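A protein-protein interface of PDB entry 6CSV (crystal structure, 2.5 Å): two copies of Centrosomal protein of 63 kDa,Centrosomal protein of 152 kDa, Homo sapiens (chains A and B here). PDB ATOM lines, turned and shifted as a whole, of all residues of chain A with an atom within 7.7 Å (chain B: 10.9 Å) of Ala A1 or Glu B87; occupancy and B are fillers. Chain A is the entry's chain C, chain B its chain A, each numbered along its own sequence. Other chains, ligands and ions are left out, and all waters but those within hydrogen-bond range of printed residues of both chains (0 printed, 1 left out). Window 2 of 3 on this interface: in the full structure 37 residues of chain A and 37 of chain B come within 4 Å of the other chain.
CE of Met A3 touches CB of Met B83, at 3.3 Å.
CG2 of Val B84 touches O of Met A3, at 3.4 Å.
N of Thr A4 touches CG2 of Val B84 (3.8 Å).
Phe A6 touches Ala B80.
OE2 of Glu B87 sits at hydrogen-bond distance from NE2 of His A2 (3.0 Å).
The side-chain carboxylate (OE2) of Glu B87 is in hydrogen-bond range of the backbone NH (N) of Ala A1, at 3.1 Å.
The side-chain carboxylate (OE1) of Glu B87 is in hydrogen-bond range of the backbone NH (N) of Met A3, at 3.2 Å.
Printed residues of chain B that touch a printed residue of chain A: Ala B80, Met B83, Val B84 and Glu B87.
Hydrophobic or aromatic side chains of chain B within 4 Å of the printed part of chain A: Ala B80, Met B83 and Val B84.
Of the 8 printed residues of chain A, 5 touch a printed residue of chain B.
Hydrophobic or aromatic side chains of chain A within 4 Å of the printed part of chain B: His A2, Met A3 and Phe A6.
Among the printed residues, 7 pairs touch across the chains.
Among the printed residues, no Asp or Glu carboxylate lies within 4 Å of a Lys or Arg side-chain nitrogen of the other chain.
Printed residues of chain B within 4 Å of Ala A1: Glu B87.
Of chain B, only Glu B87 comes within 4 Å of His A2.
Met A3 touches just these residues of chain B: Met B83 (3.3 Å), Val B84 (3.4 Å) and Glu B87 (3.2 Å).
Of chain B, only Val B84 comes within 4 Å of Thr A4.
Of the printed residues of chain B, Phe A6 touches Ala B80.
Arg A90 touches none of the printed residues of chain B.
Of the printed residues of chain A, Ala B80 touches Phe A6 (3.7 Å).
Printed residues of chain A within 4 Å of Met B83: Met A3.
Printed residues of chain A within 4 Å of Val B84: Met A3 and Thr A4.
Lys B85 touches none of the printed residues of chain A.
Ala B86 touches none of the printed residues of chain A.
The nearest residue of chain A that does not touch Glu B87 is Thr A4 (4.5 Å).
The nearest printed residue of chain A that does not touch Val B84 is Arg A5 (6.1 Å).
The guanidinium group of Arg A90 lies close to a ring nitrogen (NE2) of His A2 (3.3 Å).
The backbone carbonyl oxygen of Ala A1 sits at hydrogen-bond distance from the side-chain hydroxyl of Thr A4, 3.1 Å away.
Positions printed for both chains: 2, 3 and 90.
Of the 7 pairs that touch across the chains among the printed residues, none has its exchanged pair printed and touching as well.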
ATOM      1  N   ALA A   1      -0.982  -6.184  -0.803  1.00  0.00           N
ATOM      2  CA  ALA A   1      -0.735  -7.250  -1.828  1.00  0.00           C
ATOM      3  C   ALA A   1      -1.976  -8.085  -2.208  1.00  0.00           C
ATOM      4  O   ALA A   1      -1.827  -9.164  -2.793  1.00  0.00           O
ATOM      5  CB  ALA A   1       0.390  -8.176  -1.360  1.00  0.00           C
ATOM      6  N   HIS A   2      -3.186  -7.602  -1.910  1.00  0.00           N
ATOM      7  CA  HIS A   2      -4.404  -8.331  -2.332  1.00  0.00           C
ATOM      8  C   HIS A   2      -4.545  -8.385  -3.884  1.00  0.00           C
ATOM      9  O   HIS A   2      -4.875  -9.423  -4.468  1.00  0.00           O
ATOM     10  CB  HIS A   2      -5.729  -7.848  -1.653  1.00  0.00           C
ATOM     11  CG  HIS A   2      -5.630  -6.572  -0.866  1.00  0.00           C
ATOM     12  ND1 HIS A   2      -5.018  -6.503   0.369  1.00  0.00           N
ATOM     13  CD2 HIS A   2      -6.127  -5.333  -1.104  1.00  0.00           C
ATOM     14  CE1 HIS A   2      -5.102  -5.269   0.836  1.00  0.00           C
ATOM     15  NE2 HIS A   2      -5.772  -4.539  -0.037  1.00  0.00           N
ATOM     16  N   MET A   3      -4.248  -7.276  -4.541  1.00  0.00           N
ATOM     17  CA  MET A   3      -4.576  -7.126  -5.951  1.00  0.00           C
ATOM     18  C   MET A   3      -3.641  -7.858  -6.894  1.00  0.00           C
ATOM     19  O   MET A   3      -4.017  -8.148  -8.029  1.00  0.00           O
ATOM     20  CB  MET A   3      -4.623  -5.644  -6.313  1.00  0.00           C
ATOM     21  CG  MET A   3      -5.646  -4.848  -5.509  1.00  0.00           C
ATOM     22  SD  MET A   3      -7.270  -5.650  -5.505  1.00  0.00           S
ATOM     23  CE  MET A   3      -7.751  -5.510  -7.221  1.00  0.00           C
ATOM     24  N   THR A   4      -2.432  -8.159  -6.435  1.00  0.00           N
ATOM     25  CA  THR A   4      -1.502  -8.874  -7.260  1.00  0.00           C
ATOM     26  C   THR A   4      -1.990 -10.292  -7.417  1.00  0.00           C
ATOM     27  O   THR A   4      -1.976 -10.816  -8.519  1.00  0.00           O
ATOM     28  CB  THR A   4      -0.056  -8.787  -6.735  1.00  0.00           C
ATOM     29  OG1 THR A   4       0.014  -9.134  -5.345  1.00  0.00           O
ATOM     30  CG2 THR A   4       0.426  -7.380  -6.919  1.00  0.00           C
ATOM     31  N   ARG A   5      -2.485 -10.885  -6.339  1.00  0.00           N
ATOM     32  CA  ARG A   5      -3.174 -12.173  -6.438  1.00  0.00           C
ATOM     33  C   ARG A   5      -4.418 -12.100  -7.345  1.00  0.00           C
ATOM     34  O   ARG A   5      -4.677 -13.045  -8.098  1.00  0.00           O
ATOM     35  CB  ARG A   5      -3.599 -12.709  -5.079  1.00  0.00           C
ATOM     36  CG  ARG A   5      -4.172 -14.120  -5.174  1.00  0.00           C
ATOM     37  CD  ARG A   5      -3.734 -15.006  -4.022  1.00  0.00           C
ATOM     38  NE  ARG A   5      -4.407 -14.608  -2.784  1.00  0.00           N
ATOM     39  CZ  ARG A   5      -5.055 -15.421  -1.950  1.00  0.00           C
ATOM     40  NH1 ARG A   5      -5.124 -16.740  -2.148  1.00  0.00           N
ATOM     41  NH2 ARG A   5      -5.627 -14.901  -0.876  1.00  0.00           N
ATOM     42  N   PHE A   6      -5.167 -10.990  -7.294  1.00  0.00           N
ATOM     43  CA  PHE A   6      -6.291 -10.818  -8.197  1.00  0.00           C
ATOM     44  C   PHE A   6      -5.822 -10.883  -9.659  1.00  0.00           C
ATOM     45  O   PHE A   6      -6.417 -11.575 -10.489  1.00  0.00           O
ATOM     46  CB  PHE A   6      -7.034  -9.526  -7.847  1.00  0.00           C
ATOM     47  CG  PHE A   6      -8.302  -9.304  -8.631  1.00  0.00           C
ATOM     48  CD1 PHE A   6      -9.396 -10.101  -8.436  1.00  0.00           C
ATOM     49  CD2 PHE A   6      -8.401  -8.268  -9.532  1.00  0.00           C
ATOM     50  CE1 PHE A   6     -10.550  -9.897  -9.167  1.00  0.00           C
ATOM     51  CE2 PHE A   6      -9.547  -8.054 -10.259  1.00  0.00           C
ATOM     52  CZ  PHE A   6     -10.616  -8.884 -10.098  1.00  0.00           C
ATOM     53  N   GLU A   8      -3.059 -12.243 -10.838  1.00  0.00           N
ATOM     54  CA  GLU A   8      -2.537 -13.576 -11.166  1.00  0.00           C
ATOM     55  C   GLU A   8      -3.678 -14.525 -11.536  1.00  0.00           C
ATOM     56  O   GLU A   8      -3.595 -15.316 -12.498  1.00  0.00           O
ATOM     57  CB  GLU A   8      -1.668 -14.090 -10.011  1.00  0.00           C
ATOM     58  CG  GLU A   8      -0.326 -13.358  -9.968  1.00  0.00           C
ATOM     59  CD  GLU A   8       0.410 -13.402  -8.642  1.00  0.00           C
ATOM     60  OE1 GLU A   8      -0.050 -14.039  -7.665  1.00  0.00           O
ATOM     61  OE2 GLU A   8       1.486 -12.773  -8.594  1.00  0.00           O
ATOM     62  N   ARG A  90     -11.734  -5.112   5.980  1.00  0.00           N
ATOM     63  CA  ARG A  90     -10.485  -4.396   6.340  1.00  0.00           C
ATOM     64  C   ARG A  90     -10.713  -3.081   7.111  1.00  0.00           C
ATOM     65  O   ARG A  90      -9.817  -2.596   7.783  1.00  0.00           O
ATOM     66  CB  ARG A  90      -9.596  -4.185   5.114  1.00  0.00           C
ATOM     67  CG  ARG A  90      -8.904  -5.479   4.677  1.00  0.00           C
ATOM     68  CD  ARG A  90      -7.811  -5.281   3.628  1.00  0.00           C
ATOM     69  NE  ARG A  90      -8.250  -4.574   2.411  1.00  0.00           N
ATOM     70  CZ  ARG A  90      -8.743  -5.130   1.282  1.00  0.00           C
ATOM     71  NH1 ARG A  90      -8.941  -6.449   1.146  1.00  0.00           N
ATOM     72  NH2 ARG A  90      -9.067  -4.332   0.257  1.00  0.00           N
ATOM     73  N   HIS B   2     -13.338   2.249  -3.019  1.00  0.00           N
ATOM     74  CA  HIS B   2     -12.929   2.069  -4.439  1.00  0.00           C
ATOM     75  C   HIS B   2     -13.699   0.920  -5.121  1.00  0.00           C
ATOM     76  O   HIS B   2     -14.196   1.070  -6.234  1.00  0.00           O
ATOM     77  CB  HIS B   2     -11.402   1.829  -4.539  1.00  0.00           C
ATOM     78  CG  HIS B   2     -10.636   2.418  -3.395  1.00  0.00           C
ATOM     79  ND1 HIS B   2     -10.203   1.661  -2.326  1.00  0.00           N
ATOM     80  CD2 HIS B   2     -10.309   3.699  -3.105  1.00  0.00           C
ATOM     81  CE1 HIS B   2      -9.615   2.446  -1.440  1.00  0.00           C
ATOM     82  NE2 HIS B   2      -9.658   3.686  -1.893  1.00  0.00           N
ATOM     83  N   MET B   3     -13.813  -0.203  -4.414  1.00  0.00           N
ATOM     84  CA  MET B   3     -14.202  -1.482  -4.999  1.00  0.00           C
ATOM     85  C   MET B   3     -15.652  -1.634  -5.439  1.00  0.00           C
ATOM     86  O   MET B   3     -15.947  -2.509  -6.257  1.00  0.00           O
ATOM     87  CB  MET B   3     -13.878  -2.638  -4.037  1.00  0.00           C
ATOM     88  CG  MET B   3     -13.072  -3.753  -4.672  1.00  0.00           C
ATOM     89  SD  MET B   3     -11.483  -3.133  -5.243  1.00  0.00           S
ATOM     90  CE  MET B   3     -10.796  -2.569  -3.681  1.00  0.00           C
ATOM     91  N   GLU B  78      -6.140  -5.551 -17.900  1.00  0.00           N
ATOM     92  CA  GLU B  78      -5.689  -4.172 -17.773  1.00  0.00           C
ATOM     93  C   GLU B  78      -6.345  -3.523 -16.566  1.00  0.00           C
ATOM     94  O   GLU B  78      -5.659  -2.850 -15.809  1.00  0.00           O
ATOM     95  CB  GLU B  78      -5.924  -3.383 -19.043  1.00  0.00           C
ATOM     96  CG  GLU B  78      -5.153  -3.958 -20.218  1.00  0.00           C
ATOM     97  CD  GLU B  78      -5.299  -3.178 -21.518  1.00  0.00           C
ATOM     98  OE1 GLU B  78      -5.546  -1.956 -21.472  1.00  0.00           O
ATOM     99  OE2 GLU B  78      -5.117  -3.799 -22.589  1.00  0.00           O
ATOM    100  N   ARG B  79      -7.641  -3.764 -16.342  1.00  0.00           N
ATOM    101  CA  ARG B  79      -8.336  -3.202 -15.166  1.00  0.00           C
ATOM    102  C   ARG B  79      -7.682  -3.647 -13.865  1.00  0.00           C
ATOM    103  O   ARG B  79      -7.412  -2.823 -12.972  1.00  0.00           O
ATOM    104  CB  ARG B  79      -9.815  -3.599 -15.141  1.00  0.00           C
ATOM    105  CG  ARG B  79     -10.672  -2.756 -16.070  1.00  0.00           C
ATOM    106  CD  ARG B  79     -11.867  -3.514 -16.607  1.00  0.00           C
ATOM    107  NE  ARG B  79     -12.654  -4.183 -15.566  1.00  0.00           N
ATOM    108  CZ  ARG B  79     -13.468  -3.569 -14.689  1.00  0.00           C
ATOM    109  NH1 ARG B  79     -13.607  -2.233 -14.671  1.00  0.00           N
ATOM    110  NH2 ARG B  79     -14.155  -4.309 -13.811  1.00  0.00           N
ATOM    111  N   ALA B  80      -7.427  -4.944 -13.756  1.00  0.00           N
ATOM    112  CA  ALA B  80      -6.849  -5.494 -12.533  1.00  0.00           C
ATOM    113  C   ALA B  80      -5.445  -4.932 -12.310  1.00  0.00           C
ATOM    114  O   ALA B  80      -5.049  -4.639 -11.190  1.00  0.00           O
ATOM    115  CB  ALA B  80      -6.817  -7.007 -12.607  1.00  0.00           C
ATOM    116  N   ALA B  81      -4.711  -4.755 -13.393  1.00  0.00           N
ATOM    117  CA  ALA B  81      -3.409  -4.124 -13.344  1.00  0.00           C
ATOM    118  C   ALA B  81      -3.527  -2.708 -12.781  1.00  0.00           C
ATOM    119  O   ALA B  81      -2.815  -2.375 -11.831  1.00  0.00           O
ATOM    120  CB  ALA B  81      -2.776  -4.102 -14.737  1.00  0.00           C
ATOM    121  N   GLU B  82      -4.446  -1.903 -13.324  1.00  0.00           N
ATOM    122  CA  GLU B  82      -4.721  -0.582 -12.764  1.00  0.00           C
ATOM    123  C   GLU B  82      -5.052  -0.623 -11.266  1.00  0.00           C
ATOM    124  O   GLU B  82      -4.718   0.309 -10.547  1.00  0.00           O
ATOM    125  CB  GLU B  82      -5.823   0.172 -13.538  1.00  0.00           C
ATOM    126  CG  GLU B  82      -5.421   0.760 -14.886  1.00  0.00           C
ATOM    127  CD  GLU B  82      -4.364   1.876 -14.824  1.00  0.00           C
ATOM    128  OE1 GLU B  82      -3.926   2.308 -13.727  1.00  0.00           O
ATOM    129  OE2 GLU B  82      -3.972   2.348 -15.915  1.00  0.00           O
ATOM    130  N   MET B  83      -5.680  -1.696 -10.791  1.00  0.00           N
ATOM    131  CA  MET B  83      -5.908  -1.873  -9.345  1.00  0.00           C
ATOM    132  C   MET B  83      -4.673  -2.267  -8.532  1.00  0.00           C
ATOM    133  O   MET B  83      -4.521  -1.850  -7.402  1.00  0.00           O
ATOM    134  CB  MET B  83      -7.023  -2.873  -9.085  1.00  0.00           C
ATOM    135  CG  MET B  83      -8.334  -2.483  -9.753  1.00  0.00           C
ATOM    136  SD  MET B  83      -9.765  -2.771  -8.712  1.00  0.00           S
ATOM    137  CE  MET B  83      -9.523  -1.473  -7.499  1.00  0.00           C
ATOM    138  N   VAL B  84      -3.770  -3.039  -9.100  1.00  0.00           N
ATOM    139  CA  VAL B  84      -2.442  -3.195  -8.486  1.00  0.00           C
ATOM    140  C   VAL B  84      -1.769  -1.821  -8.275  1.00  0.00           C
ATOM    141  O   VAL B  84      -1.248  -1.531  -7.183  1.00  0.00           O
ATOM    142  CB  VAL B  84      -1.558  -4.127  -9.320  1.00  0.00           C
ATOM    143  CG1 VAL B  84      -0.079  -4.044  -8.895  1.00  0.00           C
ATOM    144  CG2 VAL B  84      -2.089  -5.550  -9.226  1.00  0.00           C
ATOM    145  N   LYS B  85      -1.832  -0.973  -9.297  1.00  0.00           N
ATOM    146  CA  LYS B  85      -1.221   0.342  -9.252  1.00  0.00           C
ATOM    147  C   LYS B  85      -1.820   1.185  -8.142  1.00  0.00           C
ATOM    148  O   LYS B  85      -1.101   1.634  -7.253  1.00  0.00           O
ATOM    149  CB  LYS B  85      -1.378   1.052 -10.595  1.00  0.00           C
ATOM    150  CG  LYS B  85      -0.405   2.188 -10.829  1.00  0.00           C
ATOM    151  CD  LYS B  85      -1.074   3.380 -11.497  1.00  0.00           C
ATOM    152  CE  LYS B  85      -0.237   3.959 -12.615  1.00  0.00           C
ATOM    153  NZ  LYS B  85       1.032   4.516 -12.091  1.00  0.00           N
ATOM    154  N   ALA B  86      -3.142   1.363  -8.170  1.00  0.00           N
ATOM    155  CA  ALA B  86      -3.857   2.193  -7.181  1.00  0.00           C
ATOM    156  C   ALA B  86      -3.757   1.629  -5.776  1.00  0.00           C
ATOM    157  O   ALA B  86      -3.767   2.395  -4.826  1.00  0.00           O
ATOM    158  CB  ALA B  86      -5.325   2.360  -7.561  1.00  0.00           C
ATOM    159  N   GLU B  87      -3.661   0.312  -5.616  1.00  0.00           N
ATOM    160  CA  GLU B  87      -3.363  -0.218  -4.285  1.00  0.00           C
ATOM    161  C   GLU B  87      -1.972   0.222  -3.874  1.00  0.00           C
ATOM    162  O   GLU B  87      -1.756   0.459  -2.695  1.00  0.00           O
ATOM    163  CB  GLU B  87      -3.476  -1.730  -4.216  1.00  0.00           C
ATOM    164  CG  GLU B  87      -3.379  -2.348  -2.823  1.00  0.00           C
ATOM    165  CD  GLU B  87      -3.161  -3.868  -2.826  1.00  0.00           C
ATOM    166  OE1 GLU B  87      -2.768  -4.464  -3.867  1.00  0.00           O
ATOM    167  OE2 GLU B  87      -3.369  -4.481  -1.763  1.00  0.00           O
ATOM    168  N   VAL B  88      -1.027   0.328  -4.819  1.00  0.00           N
ATOM    169  CA  VAL B  88       0.333   0.768  -4.499  1.00  0.00           C
ATOM    170  C   VAL B  88       0.312   2.238  -4.180  1.00  0.00           C
ATOM    171  O   VAL B  88       0.915   2.679  -3.202  1.00  0.00           O
ATOM    172  CB  VAL B  88       1.375   0.410  -5.594  1.00  0.00           C
ATOM    173  CG1 VAL B  88       2.677   1.199  -5.407  1.00  0.00           C
ATOM    174  CG2 VAL B  88       1.686  -1.084  -5.570  1.00  0.00           C
ATOM    175  N   LEU B  89      -0.393   3.012  -4.969  1.00  0.00           N
ATOM    176  CA  LEU B  89      -0.503   4.443  -4.648  1.00  0.00           C
ATOM    177  C   LEU B  89      -1.107   4.723  -3.256  1.00  0.00           C
ATOM    178  O   LEU B  89      -0.769   5.726  -2.644  1.00  0.00           O
ATOM    179  CB  LEU B  89      -1.277   5.219  -5.716  1.00  0.00           C
ATOM    180  CG  LEU B  89      -0.386   5.915  -6.736  1.00  0.00           C
ATOM    181  CD1 LEU B  89       0.443   4.932  -7.559  1.00  0.00           C
ATOM    182  CD2 LEU B  89      -1.251   6.790  -7.639  1.00  0.00           C
ATOM    183  N   ARG B  90      -1.982   3.859  -2.746  1.00  0.00           N
ATOM    184  CA  ARG B  90      -2.630   4.145  -1.465  1.00  0.00           C
ATOM    185  C   ARG B  90      -1.740   3.800  -0.253  1.00  0.00           C
ATOM    186  O   ARG B  90      -2.073   4.181   0.873  1.00  0.00           O
ATOM    187  CB  ARG B  90      -4.029   3.500  -1.372  1.00  0.00           C
ATOM    188  CG  ARG B  90      -5.102   4.233  -2.197  1.00  0.00           C
ATOM    189  CD  ARG B  90      -6.508   3.653  -2.049  1.00  0.00           C
ATOM    190  NE  ARG B  90      -6.544   2.181  -2.184  1.00  0.00           N
ATOM    191  CZ  ARG B  90      -6.934   1.477  -3.265  1.00  0.00           C
ATOM    192  NH1 ARG B  90      -7.358   2.082  -4.390  1.00  0.00           N
ATOM    193  NH2 ARG B  90      -6.901   0.128  -3.220  1.00  0.00           N
ATOM    194  N   GLU B  91      -0.606   3.118  -0.479  1.00  0.00           N
ATOM    195  CA  GLU B  91       0.393   2.894   0.589  1.00  0.00           C
ATOM    196  C   GLU B  91       1.149   4.193   0.899  1.00  0.00           C
ATOM    197  O   GLU B  91       1.774   4.295   1.939  1.00  0.00           O
ATOM    198  CB  GLU B  91       1.375   1.748   0.231  1.00  0.00           C
ATOM    199  CG  GLU B  91       0.711   0.405  -0.057  1.00  0.00           C
ATOM    200  CD  GLU B  91       1.675  -0.694  -0.511  1.00  0.00           C
ATOM    201  OE1 GLU B  91       2.491  -1.178   0.289  1.00  0.00           O
ATOM    202  OE2 GLU B  91       1.597  -1.124  -1.665  1.00  0.00           O
ATOM    203  N   ARG B  92       1.061   5.164  -0.011  1.00  0.00           N
ATOM    204  CA  ARG B  92       1.667   6.503   0.099  1.00  0.00           C
ATOM    205  C   ARG B  92       1.046   7.290   1.250  1.00  0.00           C
ATOM    206  O   ARG B  92       1.517   7.229   2.385  1.00  0.00           O
ATOM    207  CB  ARG B  92       1.450   7.263  -1.239  1.00  0.00           C
ATOM    208  CG  ARG B  92       2.507   8.285  -1.663  1.00  0.00           C
ATOM    209  CD  ARG B  92       2.788   8.254  -3.188  1.00  0.00           C
ATOM    210  NE  ARG B  92       1.952   9.153  -3.998  1.00  0.00           N
ATOM    211  CZ  ARG B  92       2.062   9.336  -5.319  1.00  0.00           C
ATOM    212  NH1 ARG B  92       1.250  10.199  -5.931  1.00  0.00           N
ATOM    213  NH2 ARG B  92       2.965   8.669  -6.041  1.00  0.00           N
